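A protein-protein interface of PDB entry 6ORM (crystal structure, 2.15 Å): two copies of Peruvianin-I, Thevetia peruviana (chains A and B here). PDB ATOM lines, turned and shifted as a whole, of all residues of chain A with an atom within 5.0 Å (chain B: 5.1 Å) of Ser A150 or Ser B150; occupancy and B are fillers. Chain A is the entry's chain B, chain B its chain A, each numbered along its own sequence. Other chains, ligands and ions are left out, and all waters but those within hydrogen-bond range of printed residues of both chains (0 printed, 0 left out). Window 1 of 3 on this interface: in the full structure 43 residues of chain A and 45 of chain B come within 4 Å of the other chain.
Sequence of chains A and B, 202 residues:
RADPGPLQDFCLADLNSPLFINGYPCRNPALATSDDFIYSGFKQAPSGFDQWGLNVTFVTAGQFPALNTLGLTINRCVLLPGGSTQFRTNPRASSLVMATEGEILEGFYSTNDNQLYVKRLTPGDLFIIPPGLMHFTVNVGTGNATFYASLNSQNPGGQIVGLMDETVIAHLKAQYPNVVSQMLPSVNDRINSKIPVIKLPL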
ATOM      1  N   LEU A  72     -28.360  -6.141  31.081  1.00  0.00           N
ATOM      2  CA  LEU A  72     -27.726  -4.930  30.578  1.00  0.00           C
ATOM      3  C   LEU A  72     -26.222  -4.959  30.811  1.00  0.00           C
ATOM      4  O   LEU A  72     -25.726  -5.580  31.755  1.00  0.00           O
ATOM      5  CB  LEU A  72     -28.308  -3.665  31.220  1.00  0.00           C
ATOM      6  CG  LEU A  72     -29.590  -3.122  30.590  1.00  0.00           C
ATOM      7  CD1 LEU A  72     -30.169  -2.031  31.472  1.00  0.00           C
ATOM      8  CD2 LEU A  72     -29.339  -2.606  29.176  1.00  0.00           C
ATOM      9  N   THR A  73     -25.510  -4.272  29.918  1.00  0.00           N
ATOM     10  CA  THR A  73     -24.072  -4.061  29.988  1.00  0.00           C
ATOM     11  C   THR A  73     -23.793  -2.672  29.441  1.00  0.00           C
ATOM     12  O   THR A  73     -24.475  -2.210  28.523  1.00  0.00           O
ATOM     13  CB  THR A  73     -23.298  -5.123  29.171  1.00  0.00           C
ATOM     14  OG1 THR A  73     -23.180  -6.334  29.927  1.00  0.00           O
ATOM     15  CG2 THR A  73     -21.899  -4.645  28.774  1.00  0.00           C
ATOM     16  N   ILE A  74     -22.805  -1.991  30.016  1.00  0.00           N
ATOM     17  CA  ILE A  74     -22.258  -0.783  29.415  1.00  0.00           C
ATOM     18  C   ILE A  74     -20.740  -0.905  29.394  1.00  0.00           C
ATOM     19  O   ILE A  74     -20.128  -1.312  30.385  1.00  0.00           O
ATOM     20  CB  ILE A  74     -22.714   0.502  30.135  1.00  0.00           C
ATOM     21  CG1 ILE A  74     -22.263   1.730  29.343  1.00  0.00           C
ATOM     22  CG2 ILE A  74     -22.202   0.560  31.561  1.00  0.00           C
ATOM     23  CD1 ILE A  74     -22.910   3.026  29.785  1.00  0.00           C
ATOM     24  N   SER A  94     -27.586  -6.308  20.900  1.00  0.00           N
ATOM     25  CA  SER A  94     -27.498  -5.013  20.250  1.00  0.00           C
ATOM     26  C   SER A  94     -26.496  -4.136  20.991  1.00  0.00           C
ATOM     27  O   SER A  94     -26.199  -4.351  22.171  1.00  0.00           O
ATOM     28  CB  SER A  94     -28.861  -4.323  20.227  1.00  0.00           C
ATOM     29  OG  SER A  94     -29.849  -5.149  19.639  1.00  0.00           O
ATOM     30  N   SER A  95     -25.973  -3.134  20.289  1.00  0.00           N
ATOM     31  CA  SER A  95     -25.092  -2.146  20.896  1.00  0.00           C
ATOM     32  C   SER A  95     -25.577  -0.755  20.522  1.00  0.00           C
ATOM     33  O   SER A  95     -25.631  -0.414  19.336  1.00  0.00           O
ATOM     34  CB  SER A  95     -23.644  -2.343  20.449  1.00  0.00           C
ATOM     35  OG  SER A  95     -22.802  -1.401  21.086  1.00  0.00           O
ATOM     36  N   LEU A  96     -25.905   0.049  21.531  1.00  0.00           N
ATOM     37  CA  LEU A  96     -26.290   1.442  21.338  1.00  0.00           C
ATOM     38  C   LEU A  96     -25.121   2.313  21.786  1.00  0.00           C
ATOM     39  O   LEU A  96     -24.825   2.404  22.982  1.00  0.00           O
ATOM     40  CB  LEU A  96     -27.564   1.766  22.114  1.00  0.00           C
ATOM     41  CG  LEU A  96     -28.127   3.185  21.993  1.00  0.00           C
ATOM     42  CD1 LEU A  96     -28.237   3.615  20.533  1.00  0.00           C
ATOM     43  CD2 LEU A  96     -29.481   3.272  22.691  1.00  0.00           C
ATOM     44  N   VAL A  97     -24.460   2.945  20.821  1.00  0.00           N
ATOM     45  CA  VAL A  97     -23.243   3.708  21.068  1.00  0.00           C
ATOM     46  C   VAL A  97     -23.602   5.168  21.300  1.00  0.00           C
ATOM     47  O   VAL A  97     -24.357   5.760  20.521  1.00  0.00           O
ATOM     48  CB  VAL A  97     -22.270   3.564  19.888  1.00  0.00           C
ATOM     49  CG1 VAL A  97     -21.115   4.544  20.023  1.00  0.00           C
ATOM     50  CG2 VAL A  97     -21.768   2.126  19.778  1.00  0.00           C
ATOM     51  N   TYR A 148     -19.580   5.302  24.835  1.00  0.00           N
ATOM     52  CA  TYR A 148     -20.105   4.242  25.682  1.00  0.00           C
ATOM     53  C   TYR A 148     -21.056   3.379  24.868  1.00  0.00           C
ATOM     54  O   TYR A 148     -21.931   3.902  24.170  1.00  0.00           O
ATOM     55  CB  TYR A 148     -20.818   4.821  26.905  1.00  0.00           C
ATOM     56  CG  TYR A 148     -19.901   5.589  27.828  1.00  0.00           C
ATOM     57  CD1 TYR A 148     -19.514   6.889  27.530  1.00  0.00           C
ATOM     58  CD2 TYR A 148     -19.423   5.013  28.997  1.00  0.00           C
ATOM     59  CE1 TYR A 148     -18.675   7.595  28.369  1.00  0.00           C
ATOM     60  CE2 TYR A 148     -18.586   5.710  29.844  1.00  0.00           C
ATOM     61  CZ  TYR A 148     -18.215   6.999  29.526  1.00  0.00           C
ATOM     62  OH  TYR A 148     -17.379   7.690  30.369  1.00  0.00           O
ATOM     63  N   ALA A 149     -20.883   2.066  24.961  1.00  0.00           N
ATOM     64  CA  ALA A 149     -21.764   1.113  24.304  1.00  0.00           C
ATOM     65  C   ALA A 149     -22.684   0.492  25.347  1.00  0.00           C
ATOM     66  O   ALA A 149     -22.214  -0.163  26.282  1.00  0.00           O
ATOM     67  CB  ALA A 149     -20.957   0.035  23.578  1.00  0.00           C
ATOM     68  N   SER A 150     -23.988   0.716  25.193  1.00  0.00           N
ATOM     69  CA  SER A 150     -25.000   0.040  25.993  1.00  0.00           C
ATOM     70  C   SER A 150     -25.490  -1.181  25.229  1.00  0.00           C
ATOM     71  O   SER A 150     -25.858  -1.076  24.053  1.00  0.00           O
ATOM     72  CB  SER A 150     -26.171   0.974  26.305  1.00  0.00           C
ATOM     73  OG  SER A 150     -25.771   2.052  27.134  1.00  0.00           O
ATOM     74  N   LEU A 151     -25.468  -2.339  25.883  1.00  0.00           N
ATOM     75  CA  LEU A 151     -25.838  -3.592  25.242  1.00  0.00           C
ATOM     76  C   LEU A 151     -26.902  -4.311  26.060  1.00  0.00           C
ATOM     77  O   LEU A 151     -26.856  -4.311  27.294  1.00  0.00           O
ATOM     78  CB  LEU A 151     -24.611  -4.486  25.057  1.00  0.00           C
ATOM     79  CG  LEU A 151     -23.462  -3.832  24.280  1.00  0.00           C
ATOM     80  CD1 LEU A 151     -22.334  -3.408  25.213  1.00  0.00           C
ATOM     81  CD2 LEU A 151     -22.941  -4.757  23.191  1.00  0.00           C
ATOM     82  N   ASN A 152     -27.854  -4.931  25.363  1.00  0.00           N
ATOM     83  CA  ASN A 152     -28.975  -5.604  26.019  1.00  0.00           C
ATOM     84  C   ASN A 152     -28.623  -7.061  26.327  1.00  0.00           C
ATOM     85  O   ASN A 152     -29.302  -8.006  25.932  1.00  0.00           O
ATOM     86  CB  ASN A 152     -30.233  -5.498  25.162  1.00  0.00           C
ATOM     87  CG  ASN A 152     -30.073  -6.141  23.794  1.00  0.00           C
ATOM     88  OD1 ASN A 152     -28.987  -6.144  23.212  1.00  0.00           O
ATOM     89  ND2 ASN A 152     -31.164  -6.696  23.276  1.00  0.00           N
ATOM     90  N   LEU B  72     -33.323  -1.769  22.887  1.00  0.00           N
ATOM     91  CA  LEU B  72     -32.568  -0.828  23.705  1.00  0.00           C
ATOM     92  C   LEU B  72     -33.187   0.563  23.677  1.00  0.00           C
ATOM     93  O   LEU B  72     -33.813   0.970  22.695  1.00  0.00           O
ATOM     94  CB  LEU B  72     -31.108  -0.740  23.247  1.00  0.00           C
ATOM     95  CG  LEU B  72     -30.199  -1.875  23.714  1.00  0.00           C
ATOM     96  CD1 LEU B  72     -28.860  -1.798  23.004  1.00  0.00           C
ATOM     97  CD2 LEU B  72     -30.016  -1.821  25.223  1.00  0.00           C
ATOM     98  N   THR B  73     -32.987   1.287  24.779  1.00  0.00           N
ATOM     99  CA  THR B  73     -33.387   2.679  24.940  1.00  0.00           C
ATOM    100  C   THR B  73     -32.335   3.363  25.804  1.00  0.00           C
ATOM    101  O   THR B  73     -31.768   2.746  26.707  1.00  0.00           O
ATOM    102  CB  THR B  73     -34.776   2.800  25.598  1.00  0.00           C
ATOM    103  OG1 THR B  73     -35.799   2.577  24.622  1.00  0.00           O
ATOM    104  CG2 THR B  73     -34.994   4.172  26.234  1.00  0.00           C
ATOM    105  N   ILE B  74     -32.060   4.635  25.515  1.00  0.00           N
ATOM    106  CA  ILE B  74     -31.289   5.478  26.421  1.00  0.00           C
ATOM    107  C   ILE B  74     -32.040   6.790  26.616  1.00  0.00           C
ATOM    108  O   ILE B  74     -32.503   7.400  25.645  1.00  0.00           O
ATOM    109  CB  ILE B  74     -29.847   5.715  25.921  1.00  0.00           C
ATOM    110  CG1 ILE B  74     -29.023   6.441  26.987  1.00  0.00           C
ATOM    111  CG2 ILE B  74     -29.821   6.469  24.601  1.00  0.00           C
ATOM    112  CD1 ILE B  74     -27.531   6.454  26.704  1.00  0.00           C
ATOM    113  N   SER B  94     -35.138  -3.240  32.824  1.00  0.00           N
ATOM    114  CA  SER B  94     -34.103  -2.793  33.741  1.00  0.00           C
ATOM    115  C   SER B  94     -33.619  -1.407  33.327  1.00  0.00           C
ATOM    116  O   SER B  94     -33.754  -0.997  32.172  1.00  0.00           O
ATOM    117  CB  SER B  94     -32.920  -3.765  33.746  1.00  0.00           C
ATOM    118  OG  SER B  94     -33.329  -5.093  34.016  1.00  0.00           O
ATOM    119  N   SER B  95     -33.039  -0.685  34.282  1.00  0.00           N
ATOM    120  CA  SER B  95     -32.446   0.618  34.008  1.00  0.00           C
ATOM    121  C   SER B  95     -31.046   0.657  34.597  1.00  0.00           C
ATOM    122  O   SER B  95     -30.874   0.476  35.806  1.00  0.00           O
ATOM    123  CB  SER B  95     -33.302   1.751  34.579  1.00  0.00           C
ATOM    124  OG  SER B  95     -32.732   3.011  34.270  1.00  0.00           O
ATOM    125  N   LEU B  96     -30.055   0.899  33.744  1.00  0.00           N
ATOM    126  CA  LEU B  96     -28.668   1.070  34.155  1.00  0.00           C
ATOM    127  C   LEU B  96     -28.343   2.557  34.062  1.00  0.00           C
ATOM    128  O   LEU B  96     -28.252   3.114  32.962  1.00  0.00           O
ATOM    129  CB  LEU B  96     -27.736   0.230  33.284  1.00  0.00           C
ATOM    130  CG  LEU B  96     -26.244   0.208  33.626  1.00  0.00           C
ATOM    131  CD1 LEU B  96     -26.020  -0.123  35.096  1.00  0.00           C
ATOM    132  CD2 LEU B  96     -25.522  -0.794  32.738  1.00  0.00           C
ATOM    133  N   VAL B  97     -28.180   3.193  35.216  1.00  0.00           N
ATOM    134  CA  VAL B  97     -27.979   4.636  35.300  1.00  0.00           C
ATOM    135  C   VAL B  97     -26.485   4.932  35.307  1.00  0.00           C
ATOM    136  O   VAL B  97     -25.725   4.299  36.047  1.00  0.00           O
ATOM    137  CB  VAL B  97     -28.651   5.207  36.560  1.00  0.00           C
ATOM    138  CG1 VAL B  97     -28.251   6.661  36.768  1.00  0.00           C
ATOM    139  CG2 VAL B  97     -30.159   5.073  36.465  1.00  0.00           C
ATOM    140  N   TYR B 148     -27.612   9.314  32.499  1.00  0.00           N
ATOM    141  CA  TYR B 148     -28.197   8.591  31.381  1.00  0.00           C
ATOM    142  C   TYR B 148     -28.677   7.232  31.862  1.00  0.00           C
ATOM    143  O   TYR B 148     -27.947   6.522  32.561  1.00  0.00           O
ATOM    144  CB  TYR B 148     -27.183   8.426  30.248  1.00  0.00           C
ATOM    145  CG  TYR B 148     -26.781   9.737  29.625  1.00  0.00           C
ATOM    146  CD1 TYR B 148     -25.838  10.556  30.230  1.00  0.00           C
ATOM    147  CD2 TYR B 148     -27.359  10.168  28.439  1.00  0.00           C
ATOM    148  CE1 TYR B 148     -25.475  11.761  29.667  1.00  0.00           C
ATOM    149  CE2 TYR B 148     -27.002  11.370  27.866  1.00  0.00           C
ATOM    150  CZ  TYR B 148     -26.060  12.162  28.486  1.00  0.00           C
ATOM    151  OH  TYR B 148     -25.700  13.363  27.923  1.00  0.00           O
ATOM    152  N   ALA B 149     -29.902   6.881  31.495  1.00  0.00           N
ATOM    153  CA  ALA B 149     -30.477   5.583  31.812  1.00  0.00           C
ATOM    154  C   ALA B 149     -30.475   4.719  30.557  1.00  0.00           C
ATOM    155  O   ALA B 149     -31.102   5.076  29.554  1.00  0.00           O
ATOM    156  CB  ALA B 149     -31.896   5.735  32.362  1.00  0.00           C
ATOM    157  N   SER B 150     -29.749   3.603  30.606  1.00  0.00           N
ATOM    158  CA  SER B 150     -29.811   2.589  29.561  1.00  0.00           C
ATOM    159  C   SER B 150     -30.814   1.524  29.982  1.00  0.00           C
ATOM    160  O   SER B 150     -30.728   0.993  31.093  1.00  0.00           O
ATOM    161  CB  SER B 150     -28.434   1.965  29.324  1.00  0.00           C
ATOM    162  OG  SER B 150     -27.514   2.917  28.814  1.00  0.00           O
ATOM    163  N   LEU B 151     -31.778   1.233  29.109  1.00  0.00           N
ATOM    164  CA  LEU B 151     -32.842   0.287  29.417  1.00  0.00           C
ATOM    165  C   LEU B 151     -32.939  -0.770  28.326  1.00  0.00           C
ATOM    166  O   LEU B 151     -32.789  -0.466  27.139  1.00  0.00           O
ATOM    167  CB  LEU B 151     -34.188   1.008  29.585  1.00  0.00           C
ATOM    168  CG  LEU B 151     -34.208   2.113  30.646  1.00  0.00           C
ATOM    169  CD1 LEU B 151     -34.147   3.497  30.003  1.00  0.00           C
ATOM    170  CD2 LEU B 151     -35.425   1.988  31.555  1.00  0.00           C
ATOM    171  N   ASN B 152     -33.198  -2.014  28.734  1.00  0.00           N
ATOM    172  CA  ASN B 152     -33.251  -3.137  27.797  1.00  0.00           C
ATOM    173  C   ASN B 152     -34.668  -3.330  27.248  1.00  0.00           C
ATOM    174  O   ASN B 152     -35.281  -4.392  27.354  1.00  0.00           O
ATOM    175  CB  ASN B 152     -32.722  -4.407  28.455  1.00  0.00           C
ATOM    176  CG  ASN B 152     -33.515  -4.809  29.684  1.00  0.00           C
ATOM    177  OD1 ASN B 152     -34.039  -3.963  30.412  1.00  0.00           O
ATOM    178  ND2 ASN B 152     -33.608  -6.114  29.921  1.00  0.00           N
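Among the printed residues, pairs that only touch across the chains: Leu A72 with Ser B150, Ser A150 with Leu B72, Asn A152 with Leu B72, Leu A72 with Leu B96, Leu A96 with Ile B74, Ser A94 with Leu B72, Ile A74 with Leu B96, Leu A96 with Leu B72, Leu A72 with Ser B94 and Leu A72 with Asn B152.
Ser A150 touches just these residues of chain B: Leu B72 and Ser B150. Ser B150 touches just these residues of chain A: Leu A72 (3.1 Å) and Ser A150 (2.6 Å). Of the printed residues of chain A, Leu B96 touches Leu A72 and Ile A74. Printed residues of chain B within 4 Å of Leu A72: Ser B94 (3.8 Å), Leu B96 (3.7 Å), Ser B150 (3.1 Å) and Asn B152 (3.9 Å). Thr A73 touches none of the printed residues of chain B. Leu A151 touches none of the printed residues of chain B. The nearest residue of chain B that does not touch Ser A150 is Ile B74 (4.8 Å). The nearest residue of chain A that does not touch Ser B150 is Ile A74 (4.7 Å). The nearest printed residue of chain A that does not touch Leu B96 is Thr A73 (4.2 Å).
Of the 12 printed residues of chain B, 6 touch a printed residue of chain A. Printed residues of chain B that touch a printed residue of chain A: Leu B72, Ile B74, Ser B94, Leu B96, Ser B150 and Asn B152. Of the 12 printed residues of chain A, 6 touch a printed residue of chain B. Printed residues of chain A that touch a printed residue of chain B: Leu A72, Ile A74, Ser A94, Leu A96, Ser A150 and Asn A152. Among the printed residues, 11 pairs touch across the chains. Among the printed residues, no Asp or Glu carboxylate lies within 4 Å of a Lys or Arg side-chain nitrogen of the other chain.
N of Ser B94 sits at hydrogen-bond distance from OD1 of Asn B152 (2.7 Å). The backbone carbonyl oxygen (O) of Ser B150 is in hydrogen-bond range of the backbone NH (N) of Leu B96. N of Ser A94 is in hydrogen-bond range of OD1 of Asn A152 (2.7 Å). The backbone NH of Leu A96 lies within hydrogen-bond range of the backbone carbonyl oxygen of Ser A150 (2.8 Å).
Leu A72 touches Leu B96, and with the chains exchanged Leu A96 touches Leu B72. Leu A72 touches Asn B152, and with the chains exchanged Asn A152 touches Leu B72. Ile A74 touches Leu B96, and with the chains exchanged Leu A96 touches Ile B74. Ser A150 touches its own counterpart, Ser B150. Positions printed for both chains: 72, 73, 74, 94, 95, 96, 97, 148, 149, 150, 151 and 152. Of the 11 pairs that touch across the chains among the printed residues, 11 have their exchanged pair printed and touching as well.
The side-chain hydroxyl (OG) of Ser A150 sits at hydrogen-bond distance from the side-chain hydroxyl (OG) of Ser B150, 2.6 Å away.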
